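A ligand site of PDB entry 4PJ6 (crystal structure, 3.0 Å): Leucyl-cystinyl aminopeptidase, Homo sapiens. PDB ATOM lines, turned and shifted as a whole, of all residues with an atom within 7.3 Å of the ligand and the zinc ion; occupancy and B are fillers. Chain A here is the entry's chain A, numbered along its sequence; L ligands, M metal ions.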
ATOM      1  N   TYR A 119      -6.139 -26.736   2.540  1.00  0.00           N
ATOM      2  CA  TYR A 119      -7.575 -26.810   2.863  1.00  0.00           C
ATOM      3  C   TYR A 119      -8.090 -28.164   2.382  1.00  0.00           C
ATOM      4  O   TYR A 119      -7.697 -28.624   1.304  1.00  0.00           O
ATOM      5  CB  TYR A 119      -8.260 -25.701   2.125  1.00  0.00           C
ATOM      6  CG  TYR A 119      -9.733 -25.478   2.388  1.00  0.00           C
ATOM      7  CD1 TYR A 119     -10.208 -25.120   3.659  1.00  0.00           C
ATOM      8  CD2 TYR A 119     -10.664 -25.531   1.323  1.00  0.00           C
ATOM      9  CE1 TYR A 119     -11.557 -24.847   3.894  1.00  0.00           C
ATOM     10  CE2 TYR A 119     -12.006 -25.269   1.540  1.00  0.00           C
ATOM     11  CZ  TYR A 119     -12.453 -24.931   2.828  1.00  0.00           C
ATOM     12  OH  TYR A 119     -13.786 -24.675   3.059  1.00  0.00           O
ATOM     13  N   GLN A 140      -8.179 -29.966   7.420  1.00  0.00           N
ATOM     14  CA  GLN A 140      -8.657 -28.646   7.772  1.00  0.00           C
ATOM     15  C   GLN A 140      -9.947 -28.538   6.985  1.00  0.00           C
ATOM     16  O   GLN A 140      -9.933 -28.256   5.788  1.00  0.00           O
ATOM     17  CB  GLN A 140      -7.650 -27.591   7.309  1.00  0.00           C
ATOM     18  CG  GLN A 140      -8.041 -26.152   7.571  1.00  0.00           C
ATOM     19  CD  GLN A 140      -8.415 -25.905   9.004  1.00  0.00           C
ATOM     20  OE1 GLN A 140      -7.626 -26.154   9.909  1.00  0.00           O
ATOM     21  NE2 GLN A 140      -9.620 -25.398   9.222  1.00  0.00           N
ATOM     22  N   PHE A 141     -11.067 -28.826   7.629  1.00  0.00           N
ATOM     23  CA  PHE A 141     -12.346 -28.903   6.909  1.00  0.00           C
ATOM     24  C   PHE A 141     -13.175 -27.628   7.090  1.00  0.00           C
ATOM     25  O   PHE A 141     -14.058 -27.349   6.273  1.00  0.00           O
ATOM     26  CB  PHE A 141     -13.208 -30.128   7.323  1.00  0.00           C
ATOM     27  CG  PHE A 141     -12.581 -31.477   7.045  1.00  0.00           C
ATOM     28  CD1 PHE A 141     -11.656 -31.671   6.020  1.00  0.00           C
ATOM     29  CD2 PHE A 141     -12.940 -32.587   7.812  1.00  0.00           C
ATOM     30  CE1 PHE A 141     -11.077 -32.913   5.798  1.00  0.00           C
ATOM     31  CE2 PHE A 141     -12.383 -33.833   7.571  1.00  0.00           C
ATOM     32  CZ  PHE A 141     -11.451 -33.996   6.564  1.00  0.00           C
ATOM     33  N   GLU A 142     -12.918 -26.874   8.170  1.00  0.00           N
ATOM     34  CA  GLU A 142     -13.714 -25.689   8.458  1.00  0.00           C
ATOM     35  C   GLU A 142     -13.402 -24.632   7.410  1.00  0.00           C
ATOM     36  O   GLU A 142     -12.225 -24.303   7.186  1.00  0.00           O
ATOM     37  CB  GLU A 142     -13.419 -25.156   9.862  1.00  0.00           C
ATOM     38  CG  GLU A 142     -14.223 -23.919  10.271  1.00  0.00           C
ATOM     39  CD  GLU A 142     -14.071 -23.528  11.739  1.00  0.00           C
ATOM     40  OE1 GLU A 142     -13.002 -23.738  12.367  1.00  0.00           O
ATOM     41  OE2 GLU A 142     -15.070 -22.991  12.285  1.00  0.00           O
ATOM     42  N   PRO A 143     -14.446 -24.121   6.735  1.00  0.00           N
ATOM     43  CA  PRO A 143     -15.862 -24.460   6.882  1.00  0.00           C
ATOM     44  C   PRO A 143     -16.416 -25.593   6.009  1.00  0.00           C
ATOM     45  O   PRO A 143     -17.033 -26.511   6.526  1.00  0.00           O
ATOM     46  CB  PRO A 143     -16.558 -23.148   6.517  1.00  0.00           C
ATOM     47  CG  PRO A 143     -15.644 -22.519   5.511  1.00  0.00           C
ATOM     48  CD  PRO A 143     -14.233 -22.968   5.832  1.00  0.00           C
ATOM     49  N   GLY A 275      -3.262 -25.634   8.264  1.00  0.00           N
ATOM     50  CA  GLY A 275      -4.568 -25.376   8.847  1.00  0.00           C
ATOM     51  C   GLY A 275      -4.593 -25.592  10.349  1.00  0.00           C
ATOM     52  O   GLY A 275      -4.471 -26.726  10.822  1.00  0.00           O
ATOM     53  N   ALA A 276      -4.752 -24.520  11.115  1.00  0.00           N
ATOM     54  CA  ALA A 276      -4.843 -24.615  12.578  1.00  0.00           C
ATOM     55  C   ALA A 276      -6.288 -24.422  13.065  1.00  0.00           C
ATOM     56  O   ALA A 276      -6.889 -23.379  12.794  1.00  0.00           O
ATOM     57  CB  ALA A 276      -3.912 -23.616  13.257  1.00  0.00           C
ATOM     58  N   MET A 277      -6.843 -25.438  13.754  1.00  0.00           N
ATOM     59  CA  MET A 277      -8.230 -25.446  14.296  1.00  0.00           C
ATOM     60  C   MET A 277      -8.517 -26.486  15.411  1.00  0.00           C
ATOM     61  O   MET A 277      -7.641 -27.270  15.769  1.00  0.00           O
ATOM     62  CB  MET A 277      -9.249 -25.662  13.186  1.00  0.00           C
ATOM     63  CG  MET A 277      -9.468 -27.129  12.902  1.00  0.00           C
ATOM     64  SD  MET A 277     -11.092 -27.285  12.194  1.00  0.00           S
ATOM     65  CE  MET A 277     -12.154 -26.627  13.537  1.00  0.00           C
ATOM     66  N   GLU A 278      -9.762 -26.452  15.916  1.00  0.00           N
ATOM     67  CA  GLU A 278     -10.170 -27.127  17.160  1.00  0.00           C
ATOM     68  C   GLU A 278     -10.832 -28.518  17.016  1.00  0.00           C
ATOM     69  O   GLU A 278     -11.680 -28.886  17.844  1.00  0.00           O
ATOM     70  CB  GLU A 278     -11.085 -26.187  17.972  1.00  0.00           C
ATOM     71  CG  GLU A 278     -12.482 -25.932  17.385  1.00  0.00           C
ATOM     72  CD  GLU A 278     -12.555 -24.812  16.365  1.00  0.00           C
ATOM     73  OE1 GLU A 278     -11.684 -23.898  16.355  1.00  0.00           O
ATOM     74  OE2 GLU A 278     -13.502 -24.821  15.559  1.00  0.00           O
ATOM     75  N   THR A 284      -5.478 -29.111  15.963  1.00  0.00           N
ATOM     76  CA  THR A 284      -4.340 -28.729  15.082  1.00  0.00           C
ATOM     77  C   THR A 284      -3.764 -27.320  15.384  1.00  0.00           C
ATOM     78  O   THR A 284      -4.458 -26.424  15.887  1.00  0.00           O
ATOM     79  CB  THR A 284      -4.677 -28.937  13.560  1.00  0.00           C
ATOM     80  OG1 THR A 284      -5.914 -28.306  13.242  1.00  0.00           O
ATOM     81  CG2 THR A 284      -4.800 -30.425  13.207  1.00  0.00           C
ATOM     82  N   ILE A 308      -3.740 -19.458  22.489  1.00  0.00           N
ATOM     83  CA  ILE A 308      -4.160 -20.391  21.437  1.00  0.00           C
ATOM     84  C   ILE A 308      -4.605 -21.778  21.979  1.00  0.00           C
ATOM     85  O   ILE A 308      -5.605 -22.364  21.479  1.00  0.00           O
ATOM     86  CB  ILE A 308      -3.083 -20.494  20.339  1.00  0.00           C
ATOM     87  CG1 ILE A 308      -3.679 -21.007  19.028  1.00  0.00           C
ATOM     88  CG2 ILE A 308      -1.913 -21.340  20.790  1.00  0.00           C
ATOM     89  CD1 ILE A 308      -2.772 -20.806  17.827  1.00  0.00           C
ATOM     90  N   HIS A 311      -8.046 -20.970  23.732  1.00  0.00           N
ATOM     91  CA  HIS A 311      -9.005 -20.742  22.691  1.00  0.00           C
ATOM     92  C   HIS A 311      -9.409 -22.102  22.177  1.00  0.00           C
ATOM     93  O   HIS A 311     -10.567 -22.476  22.276  1.00  0.00           O
ATOM     94  CB  HIS A 311      -8.423 -19.850  21.567  1.00  0.00           C
ATOM     95  CG  HIS A 311      -9.386 -19.584  20.442  1.00  0.00           C
ATOM     96  ND1 HIS A 311     -10.229 -18.498  20.426  1.00  0.00           N
ATOM     97  CD2 HIS A 311      -9.639 -20.270  19.295  1.00  0.00           C
ATOM     98  CE1 HIS A 311     -10.959 -18.522  19.322  1.00  0.00           C
ATOM     99  NE2 HIS A 311     -10.624 -19.589  18.621  1.00  0.00           N
ATOM    100  N   GLU A 312      -8.461 -22.867  21.658  1.00  0.00           N
ATOM    101  CA  GLU A 312      -8.825 -24.125  21.001  1.00  0.00           C
ATOM    102  C   GLU A 312      -9.483 -25.119  21.960  1.00  0.00           C
ATOM    103  O   GLU A 312     -10.330 -25.899  21.546  1.00  0.00           O
ATOM    104  CB  GLU A 312      -7.628 -24.770  20.237  1.00  0.00           C
ATOM    105  CG  GLU A 312      -6.909 -23.914  19.191  1.00  0.00           C
ATOM    106  CD  GLU A 312      -7.829 -23.324  18.139  1.00  0.00           C
ATOM    107  OE1 GLU A 312      -8.610 -24.072  17.523  1.00  0.00           O
ATOM    108  OE2 GLU A 312      -7.763 -22.096  17.910  1.00  0.00           O
ATOM    109  N   HIS A 315     -13.287 -24.179  22.825  1.00  0.00           N
ATOM    110  CA  HIS A 315     -14.057 -24.516  21.652  1.00  0.00           C
ATOM    111  C   HIS A 315     -14.553 -25.963  21.716  1.00  0.00           C
ATOM    112  O   HIS A 315     -15.524 -26.316  21.034  1.00  0.00           O
ATOM    113  CB  HIS A 315     -13.138 -24.405  20.437  1.00  0.00           C
ATOM    114  CG  HIS A 315     -13.288 -23.140  19.648  1.00  0.00           C
ATOM    115  ND1 HIS A 315     -14.471 -22.754  19.072  1.00  0.00           N
ATOM    116  CD2 HIS A 315     -12.360 -22.218  19.270  1.00  0.00           C
ATOM    117  CE1 HIS A 315     -14.287 -21.610  18.411  1.00  0.00           C
ATOM    118  NE2 HIS A 315     -13.012 -21.277  18.508  1.00  0.00           N
ATOM    119  N   LEU A 330     -21.311 -18.146  13.829  1.00  0.00           N
ATOM    120  CA  LEU A 330     -19.946 -18.525  14.111  1.00  0.00           C
ATOM    121  C   LEU A 330     -19.334 -17.654  15.213  1.00  0.00           C
ATOM    122  O   LEU A 330     -18.663 -18.151  16.117  1.00  0.00           O
ATOM    123  CB  LEU A 330     -19.119 -18.449  12.834  1.00  0.00           C
ATOM    124  CG  LEU A 330     -17.602 -18.687  12.941  1.00  0.00           C
ATOM    125  CD1 LEU A 330     -17.281 -20.081  13.481  1.00  0.00           C
ATOM    126  CD2 LEU A 330     -16.939 -18.468  11.583  1.00  0.00           C
ATOM    127  N   ASN A 333     -19.479 -18.782  18.830  1.00  0.00           N
ATOM    128  CA  ASN A 333     -18.537 -19.824  19.293  1.00  0.00           C
ATOM    129  C   ASN A 333     -17.074 -19.295  19.428  1.00  0.00           C
ATOM    130  O   ASN A 333     -16.374 -19.579  20.427  1.00  0.00           O
ATOM    131  CB  ASN A 333     -18.674 -21.110  18.431  1.00  0.00           C
ATOM    132  CG  ASN A 333     -19.923 -21.955  18.800  1.00  0.00           C
ATOM    133  OD1 ASN A 333     -20.372 -21.982  19.951  1.00  0.00           O
ATOM    134  ND2 ASN A 333     -20.455 -22.661  17.810  1.00  0.00           N
ATOM    135  N   GLU A 334     -16.683 -18.485  18.445  1.00  0.00           N
ATOM    136  CA  GLU A 334     -15.381 -17.836  18.364  1.00  0.00           C
ATOM    137  C   GLU A 334     -15.332 -16.673  19.307  1.00  0.00           C
ATOM    138  O   GLU A 334     -14.263 -16.333  19.849  1.00  0.00           O
ATOM    139  CB  GLU A 334     -15.075 -17.377  16.945  1.00  0.00           C
ATOM    140  CG  GLU A 334     -14.934 -18.513  15.956  1.00  0.00           C
ATOM    141  CD  GLU A 334     -13.740 -19.423  16.201  1.00  0.00           C
ATOM    142  OE1 GLU A 334     -12.798 -19.068  16.964  1.00  0.00           O
ATOM    143  OE2 GLU A 334     -13.737 -20.511  15.585  1.00  0.00           O
ATOM    144  N   GLY A 335     -16.494 -16.066  19.537  1.00  0.00           N
ATOM    145  CA  GLY A 335     -16.596 -14.988  20.495  1.00  0.00           C
ATOM    146  C   GLY A 335     -16.364 -15.559  21.878  1.00  0.00           C
ATOM    147  O   GLY A 335     -15.609 -14.984  22.659  1.00  0.00           O
ATOM    148  N   ALA A 337     -14.913 -18.563  22.695  1.00  0.00           N
ATOM    149  CA  ALA A 337     -13.546 -19.011  22.754  1.00  0.00           C
ATOM    150  C   ALA A 337     -12.632 -17.824  22.986  1.00  0.00           C
ATOM    151  O   ALA A 337     -11.829 -17.829  23.928  1.00  0.00           O
ATOM    152  CB  ALA A 337     -13.192 -19.722  21.478  1.00  0.00           C
ATOM    153  N   THR A 338     -12.760 -16.784  22.168  1.00  0.00           N
ATOM    154  CA  THR A 338     -11.946 -15.587  22.376  1.00  0.00           C
ATOM    155  C   THR A 338     -12.144 -14.916  23.752  1.00  0.00           C
ATOM    156  O   THR A 338     -11.310 -14.151  24.175  1.00  0.00           O
ATOM    157  CB  THR A 338     -12.146 -14.571  21.232  1.00  0.00           C
ATOM    158  OG1 THR A 338     -11.884 -15.234  19.989  1.00  0.00           O
ATOM    159  CG2 THR A 338     -11.200 -13.372  21.366  1.00  0.00           C
ATOM    160  N   GLU A 341     -10.487 -17.268  26.351  1.00  0.00           N
ATOM    161  CA  GLU A 341      -9.092 -17.102  26.033  1.00  0.00           C
ATOM    162  C   GLU A 341      -8.529 -16.215  27.101  1.00  0.00           C
ATOM    163  O   GLU A 341      -7.497 -16.544  27.656  1.00  0.00           O
ATOM    164  CB  GLU A 341      -8.949 -16.459  24.658  1.00  0.00           C
ATOM    165  CG  GLU A 341      -7.643 -16.616  23.937  1.00  0.00           C
ATOM    166  CD  GLU A 341      -7.678 -15.814  22.664  1.00  0.00           C
ATOM    167  OE1 GLU A 341      -7.187 -14.678  22.705  1.00  0.00           O
ATOM    168  OE2 GLU A 341      -8.266 -16.265  21.658  1.00  0.00           O
ATOM    169  N   GLU A 388     -17.346 -17.787   3.963  1.00  0.00           N
ATOM    170  CA  GLU A 388     -15.941 -17.388   4.224  1.00  0.00           C
ATOM    171  C   GLU A 388     -15.710 -15.938   4.772  1.00  0.00           C
ATOM    172  O   GLU A 388     -14.662 -15.644   5.372  1.00  0.00           O
ATOM    173  CB  GLU A 388     -15.029 -17.720   3.032  1.00  0.00           C
ATOM    174  CG  GLU A 388     -14.477 -19.149   3.081  1.00  0.00           C
ATOM    175  CD  GLU A 388     -13.191 -19.276   3.921  1.00  0.00           C
ATOM    176  OE1 GLU A 388     -13.244 -19.690   5.109  1.00  0.00           O
ATOM    177  OE2 GLU A 388     -12.105 -18.966   3.394  1.00  0.00           O
ATOM    178  N   PHE A 391     -15.362 -15.304   8.810  1.00  0.00           N
ATOM    179  CA  PHE A 391     -14.105 -15.547   9.498  1.00  0.00           C
ATOM    180  C   PHE A 391     -13.292 -14.263   9.675  1.00  0.00           C
ATOM    181  O   PHE A 391     -12.258 -14.088   9.040  1.00  0.00           O
ATOM    182  CB  PHE A 391     -13.304 -16.635   8.750  1.00  0.00           C
ATOM    183  CG  PHE A 391     -13.961 -17.973   8.781  1.00  0.00           C
ATOM    184  CD1 PHE A 391     -14.940 -18.295   7.839  1.00  0.00           C
ATOM    185  CD2 PHE A 391     -13.639 -18.892   9.763  1.00  0.00           C
ATOM    186  CE1 PHE A 391     -15.564 -19.531   7.884  1.00  0.00           C
ATOM    187  CE2 PHE A 391     -14.264 -20.132   9.798  1.00  0.00           C
ATOM    188  CZ  PHE A 391     -15.233 -20.456   8.857  1.00  0.00           C
ATOM    189  N   TYR A 396     -15.357 -11.884  15.996  1.00  0.00           N
ATOM    190  CA  TYR A 396     -14.874 -12.688  17.115  1.00  0.00           C
ATOM    191  C   TYR A 396     -14.670 -11.767  18.322  1.00  0.00           C
ATOM    192  O   TYR A 396     -15.205 -12.037  19.410  1.00  0.00           O
ATOM    193  CB  TYR A 396     -13.538 -13.380  16.769  1.00  0.00           C
ATOM    194  CG  TYR A 396     -13.562 -14.369  15.595  1.00  0.00           C
ATOM    195  CD1 TYR A 396     -14.678 -14.487  14.751  1.00  0.00           C
ATOM    196  CD2 TYR A 396     -12.419 -15.150  15.305  1.00  0.00           C
ATOM    197  CE1 TYR A 396     -14.668 -15.378  13.671  1.00  0.00           C
ATOM    198  CE2 TYR A 396     -12.408 -16.033  14.221  1.00  0.00           C
ATOM    199  CZ  TYR A 396     -13.522 -16.147  13.408  1.00  0.00           C
ATOM    200  OH  TYR A 396     -13.511 -17.029  12.324  1.00  0.00           O
HETATM  201  N1  LIG L   1     -11.633 -20.990  14.049  1.00  0.00           N
HETATM  202  C1  LIG L   1     -10.368 -21.735  13.906  1.00  0.00           C
HETATM  203  C2  LIG L   1      -9.472 -21.340  15.068  1.00  0.00           C
HETATM  204  O1  LIG L   1      -9.494 -20.182  15.474  1.00  0.00           O
HETATM  205  C3  LIG L   1      -9.668 -21.400  12.588  1.00  0.00           C
HETATM  206  C4  LIG L   1     -10.290 -22.035  11.339  1.00  0.00           C
HETATM  207  C5  LIG L   1      -9.633 -21.572  10.032  1.00  0.00           C
HETATM  208  C6  LIG L   1     -10.680 -21.365   8.934  1.00  0.00           C
HETATM  209  N2  LIG L   1     -10.129 -21.235   7.555  1.00  0.00           N
HETATM  210 ZN    ZN M   1     -11.587 -20.444  17.107  1.00  0.00          ZN
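An oxygen (O1) of the ligand lies close to a ring nitrogen (NE2) of His 311 (3.4 Å). OE2 of Glu 334 lies within salt-bridge range of N1 of the ligand, 2.6 Å away. A nitrogen (N1) of the ligand is in salt-bridge range of the side-chain carboxylate of Glu 278, 3.7 Å away. N1 of the ligand lies within salt-bridge range of OE1 of Glu 142 (3.5 Å).
The backbone carbonyl oxygen (O) of Glu 334 sits at hydrogen-bond distance from the side-chain hydroxyl (OG1) of Thr 338, at 2.6 Å. The backbone carbonyl oxygen (O) of Glu 142 is in hydrogen-bond range of the side-chain amide nitrogen (NE2) of Gln 140 (3.5 Å). The side-chain carboxylate of Glu 341 lies within hydrogen-bond range of a ring nitrogen (ND1) of His 311, at 3.2 Å. The side-chain amide oxygen (OE1) of Gln 140 sits close to the backbone carbonyl oxygen (O) of Gly 275 (3.3 Å). The side-chain carboxylate of Glu 312 sits at hydrogen-bond distance from the backbone NH of Glu 278 (3.1 Å).
The zinc ion is bound by the side-chain carboxylate of Glu 334 (1.8 Å), a ring nitrogen (NE2) of His 311 (2.0 Å) and a ring nitrogen (NE2) of His 315 (2.2 Å). Slightly farther from the zinc ion lies OE2 of Glu 334 (2.6 Å). Slightly farther from the zinc ion lies an oxygen (O1) of the ligand (2.7 Å).
Residues that only touch the zinc ion: Glu 278 (3.5 Å). Four residues have an atom within 4 Å of the zinc ion: Glu 278, His 311, His 315 and Glu 334.
Merely in contact with the ligand: Gln 140, Ala 276, Glu 312 and Phe 391. Hydrophobic or aromatic side chains that line the ligand: His 311 and Phe 391. The nearest printed residue that does not touch the ligand is Met 277 (4.1 Å).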
